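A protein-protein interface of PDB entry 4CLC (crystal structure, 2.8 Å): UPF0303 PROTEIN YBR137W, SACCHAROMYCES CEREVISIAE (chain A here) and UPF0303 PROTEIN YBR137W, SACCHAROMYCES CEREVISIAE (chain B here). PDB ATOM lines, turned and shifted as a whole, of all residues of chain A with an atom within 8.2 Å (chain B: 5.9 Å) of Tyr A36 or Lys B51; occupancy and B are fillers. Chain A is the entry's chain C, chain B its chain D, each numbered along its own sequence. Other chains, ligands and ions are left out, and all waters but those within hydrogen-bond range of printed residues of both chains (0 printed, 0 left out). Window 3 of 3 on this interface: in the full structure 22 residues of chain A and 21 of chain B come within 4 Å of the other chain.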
ATOM      1  N   THR A  33     -10.539  10.761   6.247  1.00  0.00           N
ATOM      2  CA  THR A  33      -9.424  11.670   6.097  1.00  0.00           C
ATOM      3  C   THR A  33      -8.709  11.368   4.792  1.00  0.00           C
ATOM      4  O   THR A  33      -8.752  10.231   4.315  1.00  0.00           O
ATOM      5  CB  THR A  33      -8.430  11.549   7.256  1.00  0.00           C
ATOM      6  OG1 THR A  33      -7.795  10.261   7.204  1.00  0.00           O
ATOM      7  CG2 THR A  33      -9.155  11.722   8.582  1.00  0.00           C
ATOM      8  N   PHE A  34      -8.082  12.395   4.206  1.00  0.00           N
ATOM      9  CA  PHE A  34      -7.129  12.197   3.109  1.00  0.00           C
ATOM     10  C   PHE A  34      -5.808  12.925   3.372  1.00  0.00           C
ATOM     11  O   PHE A  34      -5.701  14.154   3.262  1.00  0.00           O
ATOM     12  CB  PHE A  34      -7.725  12.655   1.779  1.00  0.00           C
ATOM     13  CG  PHE A  34      -7.066  12.039   0.593  1.00  0.00           C
ATOM     14  CD1 PHE A  34      -6.893  10.669   0.525  1.00  0.00           C
ATOM     15  CD2 PHE A  34      -6.611  12.825  -0.457  1.00  0.00           C
ATOM     16  CE1 PHE A  34      -6.271  10.093  -0.568  1.00  0.00           C
ATOM     17  CE2 PHE A  34      -5.986  12.251  -1.554  1.00  0.00           C
ATOM     18  CZ  PHE A  34      -5.820  10.884  -1.615  1.00  0.00           C
ATOM     19  N   THR A  35      -4.786  12.124   3.630  1.00  0.00           N
ATOM     20  CA  THR A  35      -3.507  12.574   4.160  1.00  0.00           C
ATOM     21  C   THR A  35      -2.429  12.087   3.218  1.00  0.00           C
ATOM     22  O   THR A  35      -2.659  11.111   2.520  1.00  0.00           O
ATOM     23  CB  THR A  35      -3.329  12.031   5.621  1.00  0.00           C
ATOM     24  OG1 THR A  35      -3.749  13.026   6.561  1.00  0.00           O
ATOM     25  CG2 THR A  35      -1.925  11.560   5.932  1.00  0.00           C
ATOM     26  N   TYR A  36      -1.276  12.756   3.161  1.00  0.00           N
ATOM     27  CA  TYR A  36      -0.187  12.312   2.283  1.00  0.00           C
ATOM     28  C   TYR A  36       0.132  10.840   2.536  1.00  0.00           C
ATOM     29  O   TYR A  36       0.587  10.114   1.643  1.00  0.00           O
ATOM     30  CB  TYR A  36       1.081  13.142   2.503  1.00  0.00           C
ATOM     31  CG  TYR A  36       1.890  12.637   3.676  1.00  0.00           C
ATOM     32  CD1 TYR A  36       1.576  13.022   4.973  1.00  0.00           C
ATOM     33  CD2 TYR A  36       2.932  11.730   3.494  1.00  0.00           C
ATOM     34  CE1 TYR A  36       2.284  12.540   6.054  1.00  0.00           C
ATOM     35  CE2 TYR A  36       3.642  11.239   4.574  1.00  0.00           C
ATOM     36  CZ  TYR A  36       3.319  11.652   5.854  1.00  0.00           C
ATOM     37  OH  TYR A  36       4.035  11.172   6.931  1.00  0.00           O
ATOM     38  N   GLN A  37      -0.071  10.416   3.778  1.00  0.00           N
ATOM     39  CA  GLN A  37       0.218   9.049   4.171  1.00  0.00           C
ATOM     40  C   GLN A  37      -0.906   8.141   3.697  1.00  0.00           C
ATOM     41  O   GLN A  37      -0.682   7.003   3.277  1.00  0.00           O
ATOM     42  CB  GLN A  37       0.388   8.953   5.681  1.00  0.00           C
ATOM     43  CG  GLN A  37       0.944   7.649   6.109  1.00  0.00           C
ATOM     44  CD  GLN A  37       2.108   7.256   5.250  1.00  0.00           C
ATOM     45  OE1 GLN A  37       3.146   7.926   5.244  1.00  0.00           O
ATOM     46  NE2 GLN A  37       1.948   6.169   4.502  1.00  0.00           N
ATOM     47  N   ASP A  38      -2.121   8.670   3.764  1.00  0.00           N
ATOM     48  CA  ASP A  38      -3.268   7.971   3.246  1.00  0.00           C
ATOM     49  C   ASP A  38      -3.058   7.642   1.776  1.00  0.00           C
ATOM     50  O   ASP A  38      -3.299   6.505   1.345  1.00  0.00           O
ATOM     51  CB  ASP A  38      -4.524   8.804   3.452  1.00  0.00           C
ATOM     52  CG  ASP A  38      -4.938   8.864   4.902  1.00  0.00           C
ATOM     53  OD1 ASP A  38      -4.611   7.915   5.651  1.00  0.00           O
ATOM     54  OD2 ASP A  38      -5.602   9.848   5.282  1.00  0.00           O
ATOM     55  N   ALA A  39      -2.575   8.624   1.015  1.00  0.00           N
ATOM     56  CA  ALA A  39      -2.329   8.433  -0.411  1.00  0.00           C
ATOM     57  C   ALA A  39      -1.281   7.352  -0.621  1.00  0.00           C
ATOM     58  O   ALA A  39      -1.386   6.534  -1.538  1.00  0.00           O
ATOM     59  CB  ALA A  39      -1.896   9.727  -1.055  1.00  0.00           C
ATOM     60  N   PHE A  40      -0.274   7.327   0.241  1.00  0.00           N
ATOM     61  CA  PHE A  40       0.783   6.345   0.061  1.00  0.00           C
ATOM     62  C   PHE A  40       0.248   4.964   0.389  1.00  0.00           C
ATOM     63  O   PHE A  40       0.544   3.991  -0.313  1.00  0.00           O
ATOM     64  CB  PHE A  40       2.020   6.660   0.917  1.00  0.00           C
ATOM     65  CG  PHE A  40       3.128   5.666   0.732  1.00  0.00           C
ATOM     66  CD1 PHE A  40       3.819   5.603  -0.462  1.00  0.00           C
ATOM     67  CD2 PHE A  40       3.443   4.748   1.730  1.00  0.00           C
ATOM     68  CE1 PHE A  40       4.814   4.654  -0.651  1.00  0.00           C
ATOM     69  CE2 PHE A  40       4.441   3.799   1.535  1.00  0.00           C
ATOM     70  CZ  PHE A  40       5.123   3.759   0.353  1.00  0.00           C
ATOM     71  N   ASP A  41      -0.552   4.886   1.447  1.00  0.00           N
ATOM     72  CA  ASP A  41      -1.049   3.606   1.915  1.00  0.00           C
ATOM     73  C   ASP A  41      -2.003   3.008   0.903  1.00  0.00           C
ATOM     74  O   ASP A  41      -1.895   1.829   0.530  1.00  0.00           O
ATOM     75  CB  ASP A  41      -1.734   3.761   3.271  1.00  0.00           C
ATOM     76  CG  ASP A  41      -0.741   3.970   4.407  1.00  0.00           C
ATOM     77  OD1 ASP A  41       0.418   3.496   4.266  1.00  0.00           O
ATOM     78  OD2 ASP A  41      -1.126   4.601   5.429  1.00  0.00           O
ATOM     79  N   LEU A  42      -2.932   3.836   0.446  1.00  0.00           N
ATOM     80  CA  LEU A  42      -3.925   3.381  -0.502  1.00  0.00           C
ATOM     81  C   LEU A  42      -3.272   2.965  -1.816  1.00  0.00           C
ATOM     82  O   LEU A  42      -3.613   1.925  -2.393  1.00  0.00           O
ATOM     83  CB  LEU A  42      -4.955   4.468  -0.728  1.00  0.00           C
ATOM     84  CG  LEU A  42      -5.825   4.212  -1.947  1.00  0.00           C
ATOM     85  CD1 LEU A  42      -6.650   2.930  -1.784  1.00  0.00           C
ATOM     86  CD2 LEU A  42      -6.680   5.444  -2.243  1.00  0.00           C
ATOM     87  N   GLY A  43      -2.325   3.784  -2.274  1.00  0.00           N
ATOM     88  CA  GLY A  43      -1.577   3.501  -3.479  1.00  0.00           C
ATOM     89  C   GLY A  43      -0.853   2.177  -3.423  1.00  0.00           C
ATOM     90  O   GLY A  43      -0.789   1.477  -4.422  1.00  0.00           O
ATOM     91  N   ILE A  63      -2.541   8.289  -8.141  1.00  0.00           N
ATOM     92  CA  ILE A  63      -3.435   9.112  -7.334  1.00  0.00           C
ATOM     93  C   ILE A  63      -3.036  10.574  -7.416  1.00  0.00           C
ATOM     94  O   ILE A  63      -1.930  10.927  -7.053  1.00  0.00           O
ATOM     95  CB  ILE A  63      -3.457   8.685  -5.863  1.00  0.00           C
ATOM     96  CG1 ILE A  63      -3.831   7.209  -5.732  1.00  0.00           C
ATOM     97  CG2 ILE A  63      -4.457   9.531  -5.087  1.00  0.00           C
ATOM     98  CD1 ILE A  63      -3.675   6.661  -4.326  1.00  0.00           C
ATOM     99  N   HIS A  69      -1.760  17.773  -8.992  1.00  0.00           N
ATOM    100  CA  HIS A  69      -0.612  17.391  -8.174  1.00  0.00           C
ATOM    101  C   HIS A  69      -0.607  15.884  -7.959  1.00  0.00           C
ATOM    102  O   HIS A  69      -1.509  15.343  -7.360  1.00  0.00           O
ATOM    103  CB  HIS A  69      -0.650  18.129  -6.828  1.00  0.00           C
ATOM    104  CG  HIS A  69       0.437  17.723  -5.875  1.00  0.00           C
ATOM    105  ND1 HIS A  69       1.663  17.243  -6.294  1.00  0.00           N
ATOM    106  CD2 HIS A  69       0.484  17.736  -4.521  1.00  0.00           C
ATOM    107  CE1 HIS A  69       2.406  16.961  -5.245  1.00  0.00           C
ATOM    108  NE2 HIS A  69       1.722  17.256  -4.152  1.00  0.00           N
ATOM    109  N   LEU A  71       0.388  12.520  -6.273  1.00  0.00           N
ATOM    110  CA  LEU A  71       0.756  12.025  -4.956  1.00  0.00           C
ATOM    111  C   LEU A  71       1.418  10.664  -5.037  1.00  0.00           C
ATOM    112  O   LEU A  71       2.435  10.416  -4.408  1.00  0.00           O
ATOM    113  CB  LEU A  71      -0.457  11.958  -4.045  1.00  0.00           C
ATOM    114  CG  LEU A  71      -1.237  13.250  -3.778  1.00  0.00           C
ATOM    115  CD1 LEU A  71      -2.331  12.997  -2.747  1.00  0.00           C
ATOM    116  CD2 LEU A  71      -0.335  14.361  -3.327  1.00  0.00           C
ATOM    117  N   PHE A  72       0.753   9.725  -5.685  1.00  0.00           N
ATOM    118  CA  PHE A  72       1.301   8.384  -5.824  1.00  0.00           C
ATOM    119  C   PHE A  72       1.359   7.974  -7.283  1.00  0.00           C
ATOM    120  O   PHE A  72       0.434   8.243  -8.035  1.00  0.00           O
ATOM    121  CB  PHE A  72       0.453   7.383  -5.026  1.00  0.00           C
ATOM    122  CG  PHE A  72       0.939   5.976  -5.118  1.00  0.00           C
ATOM    123  CD1 PHE A  72       1.941   5.525  -4.288  1.00  0.00           C
ATOM    124  CD2 PHE A  72       0.404   5.104  -6.041  1.00  0.00           C
ATOM    125  CE1 PHE A  72       2.395   4.231  -4.382  1.00  0.00           C
ATOM    126  CE2 PHE A  72       0.866   3.812  -6.130  1.00  0.00           C
ATOM    127  CZ  PHE A  72       1.858   3.380  -5.301  1.00  0.00           C
ATOM    128  N   ILE B  46      14.471   5.742  -0.839  1.00  0.00           N
ATOM    129  CA  ILE B  46      14.628   7.184  -0.774  1.00  0.00           C
ATOM    130  C   ILE B  46      13.521   7.831   0.030  1.00  0.00           C
ATOM    131  O   ILE B  46      13.746   8.829   0.715  1.00  0.00           O
ATOM    132  CB  ILE B  46      14.639   7.804  -2.187  1.00  0.00           C
ATOM    133  CG1 ILE B  46      15.726   7.159  -3.038  1.00  0.00           C
ATOM    134  CG2 ILE B  46      14.806   9.313  -2.124  1.00  0.00           C
ATOM    135  CD1 ILE B  46      15.739   7.686  -4.410  1.00  0.00           C
ATOM    136  N   ARG B  47      12.319   7.275  -0.060  1.00  0.00           N
ATOM    137  CA  ARG B  47      11.191   7.904   0.604  1.00  0.00           C
ATOM    138  C   ARG B  47      11.427   7.799   2.089  1.00  0.00           C
ATOM    139  O   ARG B  47      11.204   8.757   2.832  1.00  0.00           O
ATOM    140  CB  ARG B  47       9.854   7.263   0.215  1.00  0.00           C
ATOM    141  CG  ARG B  47       8.642   7.985   0.826  1.00  0.00           C
ATOM    142  CD  ARG B  47       7.344   7.284   0.494  1.00  0.00           C
ATOM    143  NE  ARG B  47       6.211   7.932   1.134  1.00  0.00           N
ATOM    144  CZ  ARG B  47       5.812   7.648   2.364  1.00  0.00           C
ATOM    145  NH1 ARG B  47       6.476   6.735   3.061  1.00  0.00           N
ATOM    146  NH2 ARG B  47       4.770   8.271   2.901  1.00  0.00           N
ATOM    147  N   ASN B  48      11.901   6.634   2.510  1.00  0.00           N
ATOM    148  CA  ASN B  48      12.233   6.413   3.906  1.00  0.00           C
ATOM    149  C   ASN B  48      13.344   7.386   4.296  1.00  0.00           C
ATOM    150  O   ASN B  48      13.202   8.175   5.241  1.00  0.00           O
ATOM    151  CB  ASN B  48      12.660   4.962   4.140  1.00  0.00           C
ATOM    152  CG  ASN B  48      13.471   4.793   5.413  1.00  0.00           C
ATOM    153  OD1 ASN B  48      14.657   4.437   5.371  1.00  0.00           O
ATOM    154  ND2 ASN B  48      12.824   5.012   6.559  1.00  0.00           N
ATOM    155  N   ALA B  49      14.430   7.342   3.528  1.00  0.00           N
ATOM    156  CA  ALA B  49      15.584   8.212   3.732  1.00  0.00           C
ATOM    157  C   ALA B  49      15.206   9.685   3.910  1.00  0.00           C
ATOM    158  O   ALA B  49      15.504  10.266   4.950  1.00  0.00           O
ATOM    159  CB  ALA B  49      16.547   8.057   2.608  1.00  0.00           C
ATOM    160  N   VAL B  50      14.565  10.289   2.912  1.00  0.00           N
ATOM    161  CA  VAL B  50      14.155  11.682   3.046  1.00  0.00           C
ATOM    162  C   VAL B  50      13.327  11.878   4.310  1.00  0.00           C
ATOM    163  O   VAL B  50      13.401  12.926   4.952  1.00  0.00           O
ATOM    164  CB  VAL B  50      13.354  12.197   1.798  1.00  0.00           C
ATOM    165  CG1 VAL B  50      12.686  13.522   2.070  1.00  0.00           C
ATOM    166  CG2 VAL B  50      14.274  12.365   0.614  1.00  0.00           C
ATOM    167  N   LYS B  51      12.533  10.888   4.701  1.00  0.00           N
ATOM    168  CA  LYS B  51      11.676  11.178   5.833  1.00  0.00           C
ATOM    169  C   LYS B  51      12.391  10.978   7.175  1.00  0.00           C
ATOM    170  O   LYS B  51      12.022  11.605   8.173  1.00  0.00           O
ATOM    171  CB  LYS B  51      10.368  10.388   5.771  1.00  0.00           C
ATOM    172  CG  LYS B  51       9.166  11.375   5.873  1.00  0.00           C
ATOM    173  CD  LYS B  51       7.876  10.749   6.386  1.00  0.00           C
ATOM    174  CE  LYS B  51       7.589   9.436   5.720  1.00  0.00           C
ATOM    175  NZ  LYS B  51       6.585   8.705   6.531  1.00  0.00           N
ATOM    176  N   GLU B  52      13.415  10.135   7.207  1.00  0.00           N
ATOM    177  CA  GLU B  52      14.224  10.030   8.416  1.00  0.00           C
ATOM    178  C   GLU B  52      15.081  11.277   8.587  1.00  0.00           C
ATOM    179  O   GLU B  52      15.007  11.950   9.620  1.00  0.00           O
ATOM    180  CB  GLU B  52      15.102   8.776   8.396  1.00  0.00           C
ATOM    181  CG  GLU B  52      14.454   7.574   9.074  1.00  0.00           C
ATOM    182  CD  GLU B  52      15.045   6.251   8.611  1.00  0.00           C
ATOM    183  OE1 GLU B  52      16.252   6.214   8.293  1.00  0.00           O
ATOM    184  OE2 GLU B  52      14.298   5.248   8.557  1.00  0.00           O
ATOM    185  N   ASN B  53      15.860  11.606   7.562  1.00  0.00           N
ATOM    186  CA  ASN B  53      16.711  12.792   7.589  1.00  0.00           C
ATOM    187  C   ASN B  53      15.984  14.140   7.632  1.00  0.00           C
ATOM    188  O   ASN B  53      16.466  15.077   8.270  1.00  0.00           O
ATOM    189  CB  ASN B  53      17.648  12.782   6.388  1.00  0.00           C
ATOM    190  CG  ASN B  53      18.581  11.595   6.396  1.00  0.00           C
ATOM    191  OD1 ASN B  53      19.731  11.702   6.828  1.00  0.00           O
ATOM    192  ND2 ASN B  53      18.092  10.449   5.925  1.00  0.00           N
ATOM    193  N   PHE B  54      14.841  14.260   6.962  1.00  0.00           N
ATOM    194  CA  PHE B  54      14.148  15.544   6.953  1.00  0.00           C
ATOM    195  C   PHE B  54      12.678  15.470   7.322  1.00  0.00           C
ATOM    196  O   PHE B  54      11.825  15.901   6.533  1.00  0.00           O
ATOM    197  CB  PHE B  54      14.271  16.198   5.587  1.00  0.00           C
ATOM    198  CG  PHE B  54      15.656  16.620   5.245  1.00  0.00           C
ATOM    199  CD1 PHE B  54      16.542  15.722   4.667  1.00  0.00           C
ATOM    200  CD2 PHE B  54      16.076  17.921   5.498  1.00  0.00           C
ATOM    201  CE1 PHE B  54      17.827  16.110   4.352  1.00  0.00           C
ATOM    202  CE2 PHE B  54      17.347  18.320   5.178  1.00  0.00           C
ATOM    203  CZ  PHE B  54      18.230  17.411   4.602  1.00  0.00           C
ATOM    204  N   PRO B  55      12.378  14.982   8.543  1.00  0.00           N
ATOM    205  CA  PRO B  55      10.983  14.857   8.989  1.00  0.00           C
ATOM    206  C   PRO B  55      10.301  16.195   8.904  1.00  0.00           C
ATOM    207  O   PRO B  55      10.943  17.216   9.158  1.00  0.00           O
ATOM    208  CB  PRO B  55      11.114  14.415  10.444  1.00  0.00           C
ATOM    209  CG  PRO B  55      12.454  14.971  10.858  1.00  0.00           C
ATOM    210  CD  PRO B  55      13.325  14.799   9.660  1.00  0.00           C
ATOM    211  N   GLU B  56       9.031  16.181   8.534  1.00  0.00           N
ATOM    212  CA  GLU B  56       8.230  17.392   8.409  1.00  0.00           C
ATOM    213  C   GLU B  56       8.691  18.354   7.316  1.00  0.00           C
ATOM    214  O   GLU B  56       8.346  19.535   7.347  1.00  0.00           O
ATOM    215  CB  GLU B  56       8.190  18.118   9.752  1.00  0.00           C
ATOM    216  CG  GLU B  56       7.605  17.254  10.848  1.00  0.00           C
ATOM    217  CD  GLU B  56       7.273  18.035  12.086  1.00  0.00           C
ATOM    218  OE1 GLU B  56       8.000  19.013  12.382  1.00  0.00           O
ATOM    219  OE2 GLU B  56       6.279  17.674  12.758  1.00  0.00           O
ATOM    220  N   LYS B  57       9.428  17.830   6.333  1.00  0.00           N
ATOM    221  CA  LYS B  57       9.698  18.533   5.071  1.00  0.00           C
ATOM    222  C   LYS B  57       8.986  17.819   3.918  1.00  0.00           C
ATOM    223  O   LYS B  57       9.269  16.652   3.636  1.00  0.00           O
ATOM    224  CB  LYS B  57      11.208  18.614   4.800  1.00  0.00           C
ATOM    225  CG  LYS B  57      11.929  19.746   5.543  1.00  0.00           C
ATOM    226  CD  LYS B  57      11.539  21.104   4.995  1.00  0.00           C
ATOM    227  CE  LYS B  57      12.180  22.246   5.755  1.00  0.00           C
ATOM    228  NZ  LYS B  57      11.779  23.565   5.149  1.00  0.00           N
ATOM    229  N   VAL B  75       5.062  11.539  -2.391  1.00  0.00           N
ATOM    230  CA  VAL B  75       5.125  12.803  -1.715  1.00  0.00           C
ATOM    231  C   VAL B  75       5.462  12.442  -0.258  1.00  0.00           C
ATOM    232  O   VAL B  75       4.817  11.559   0.309  1.00  0.00           O
ATOM    233  CB  VAL B  75       3.783  13.560  -1.918  1.00  0.00           C
ATOM    234  CG1 VAL B  75       3.231  14.129  -0.633  1.00  0.00           C
ATOM    235  CG2 VAL B  75       3.930  14.613  -2.991  1.00  0.00           C
ATOM    236  N   THR B  76       6.493  13.054   0.332  1.00  0.00           N
ATOM    237  CA  THR B  76       7.059  12.537   1.604  1.00  0.00           C
ATOM    238  C   THR B  76       6.348  12.988   2.867  1.00  0.00           C
ATOM    239  O   THR B  76       6.585  12.442   3.946  1.00  0.00           O
ATOM    240  CB  THR B  76       8.544  12.927   1.812  1.00  0.00           C
ATOM    241  OG1 THR B  76       8.667  14.355   1.845  1.00  0.00           O
ATOM    242  CG2 THR B  76       9.423  12.351   0.728  1.00  0.00           C
ATOM    243  N   TYR B  77       5.469  13.971   2.727  1.00  0.00           N
ATOM    244  CA  TYR B  77       4.838  14.586   3.879  1.00  0.00           C
ATOM    245  C   TYR B  77       3.821  15.590   3.373  1.00  0.00           C
ATOM    246  O   TYR B  77       3.849  15.964   2.198  1.00  0.00           O
ATOM    247  CB  TYR B  77       5.883  15.271   4.753  1.00  0.00           C
ATOM    248  CG  TYR B  77       5.458  15.580   6.167  1.00  0.00           C
ATOM    249  CD1 TYR B  77       5.520  14.607   7.153  1.00  0.00           C
ATOM    250  CD2 TYR B  77       5.032  16.847   6.524  1.00  0.00           C
ATOM    251  CE1 TYR B  77       5.155  14.876   8.444  1.00  0.00           C
ATOM    252  CE2 TYR B  77       4.659  17.121   7.820  1.00  0.00           C
ATOM    253  CZ  TYR B  77       4.732  16.125   8.777  1.00  0.00           C
ATOM    254  OH  TYR B  77       4.377  16.373  10.078  1.00  0.00           O
ATOM    255  N   GLY B  78       2.928  16.020   4.257  1.00  0.00           N
ATOM    256  CA  GLY B  78       1.924  17.002   3.915  1.00  0.00           C
ATOM    257  C   GLY B  78       2.522  18.335   3.514  1.00  0.00           C
ATOM    258  O   GLY B  78       3.693  18.635   3.790  1.00  0.00           O
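NE2 of Gln A37 is in hydrogen-bond range of OD1 of Asp A41 (3.1 Å). N of Leu A71 is in hydrogen-bond range of O of Ile A63. The backbone carbonyl oxygen (O) of Lys B57 lies within hydrogen-bond range of the side-chain hydroxyl (OG1) of Thr B76 (3.0 Å).
Tyr A36 touches just these residues of chain B: Arg B47 (3.6 Å), Lys B51 (3.6 Å), Val B75 (3.7 Å), Thr B76 (3.2 Å), Tyr B77 (3.5 Å) and Gly B78 (3.4 Å). Of chain A, only Tyr A36 and Gln A37 come within 4 Å of Lys B51. Of the printed residues of chain A, Val B75 touches Tyr A36, His A69 and Leu A71. Of the printed residues of chain B, Gln A37 touches Arg B47 and Lys B51. Lys B57 touches none of the printed residues of chain A. Thr A33 touches none of the printed residues of chain B. The nearest printed residue of chain B that does not touch Tyr A36 is Glu B56 (7.3 Å). The nearest residue of chain A that does not touch Lys B51 is Phe A40 (7.0 Å).
OE1 of Gln A37 lies within hydrogen-bond range of NH2 of Arg B47, 2.9 Å away. The backbone carbonyl oxygen of Leu A71 sits at hydrogen-bond distance from the backbone NH of Val B75 (3.5 Å).
Among the printed residues, merely in contact across the chains: Tyr A36 with Arg B47 (3.6 Å), Tyr A36 with Lys B51 (3.6 Å), Tyr A36 with Val B75 (3.7 Å), Tyr A36 with Thr B76 (3.2 Å), Tyr A36 with Tyr B77 (3.5 Å), Tyr A36 with Gly B78 (3.4 Å), Gln A37 with Lys B51 (3.8 Å), Phe A40 with Arg B47 (3.7 Å) and His A69 with Val B75 (3.6 Å).
Of the 15 printed residues of chain A, 5 touch a printed residue of chain B. Printed residues of chain A that touch a printed residue of chain B: Tyr A36, Gln A37, Phe A40, His A69 and Leu A71. Hydrophobic or aromatic side chains of chain A within 4 Å of the printed part of chain B: Tyr A36, Phe A40 and His A69. Hydrophobic or aromatic side chains of chain B within 4 Å of the printed part of chain A: Val B75 and Tyr B77. Among the printed residues, 11 pairs touch across the chains. Among the printed residues, no Asp or Glu carboxylate lies within 4 Å of a Lys or Arg side-chain nitrogen of the other chain.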
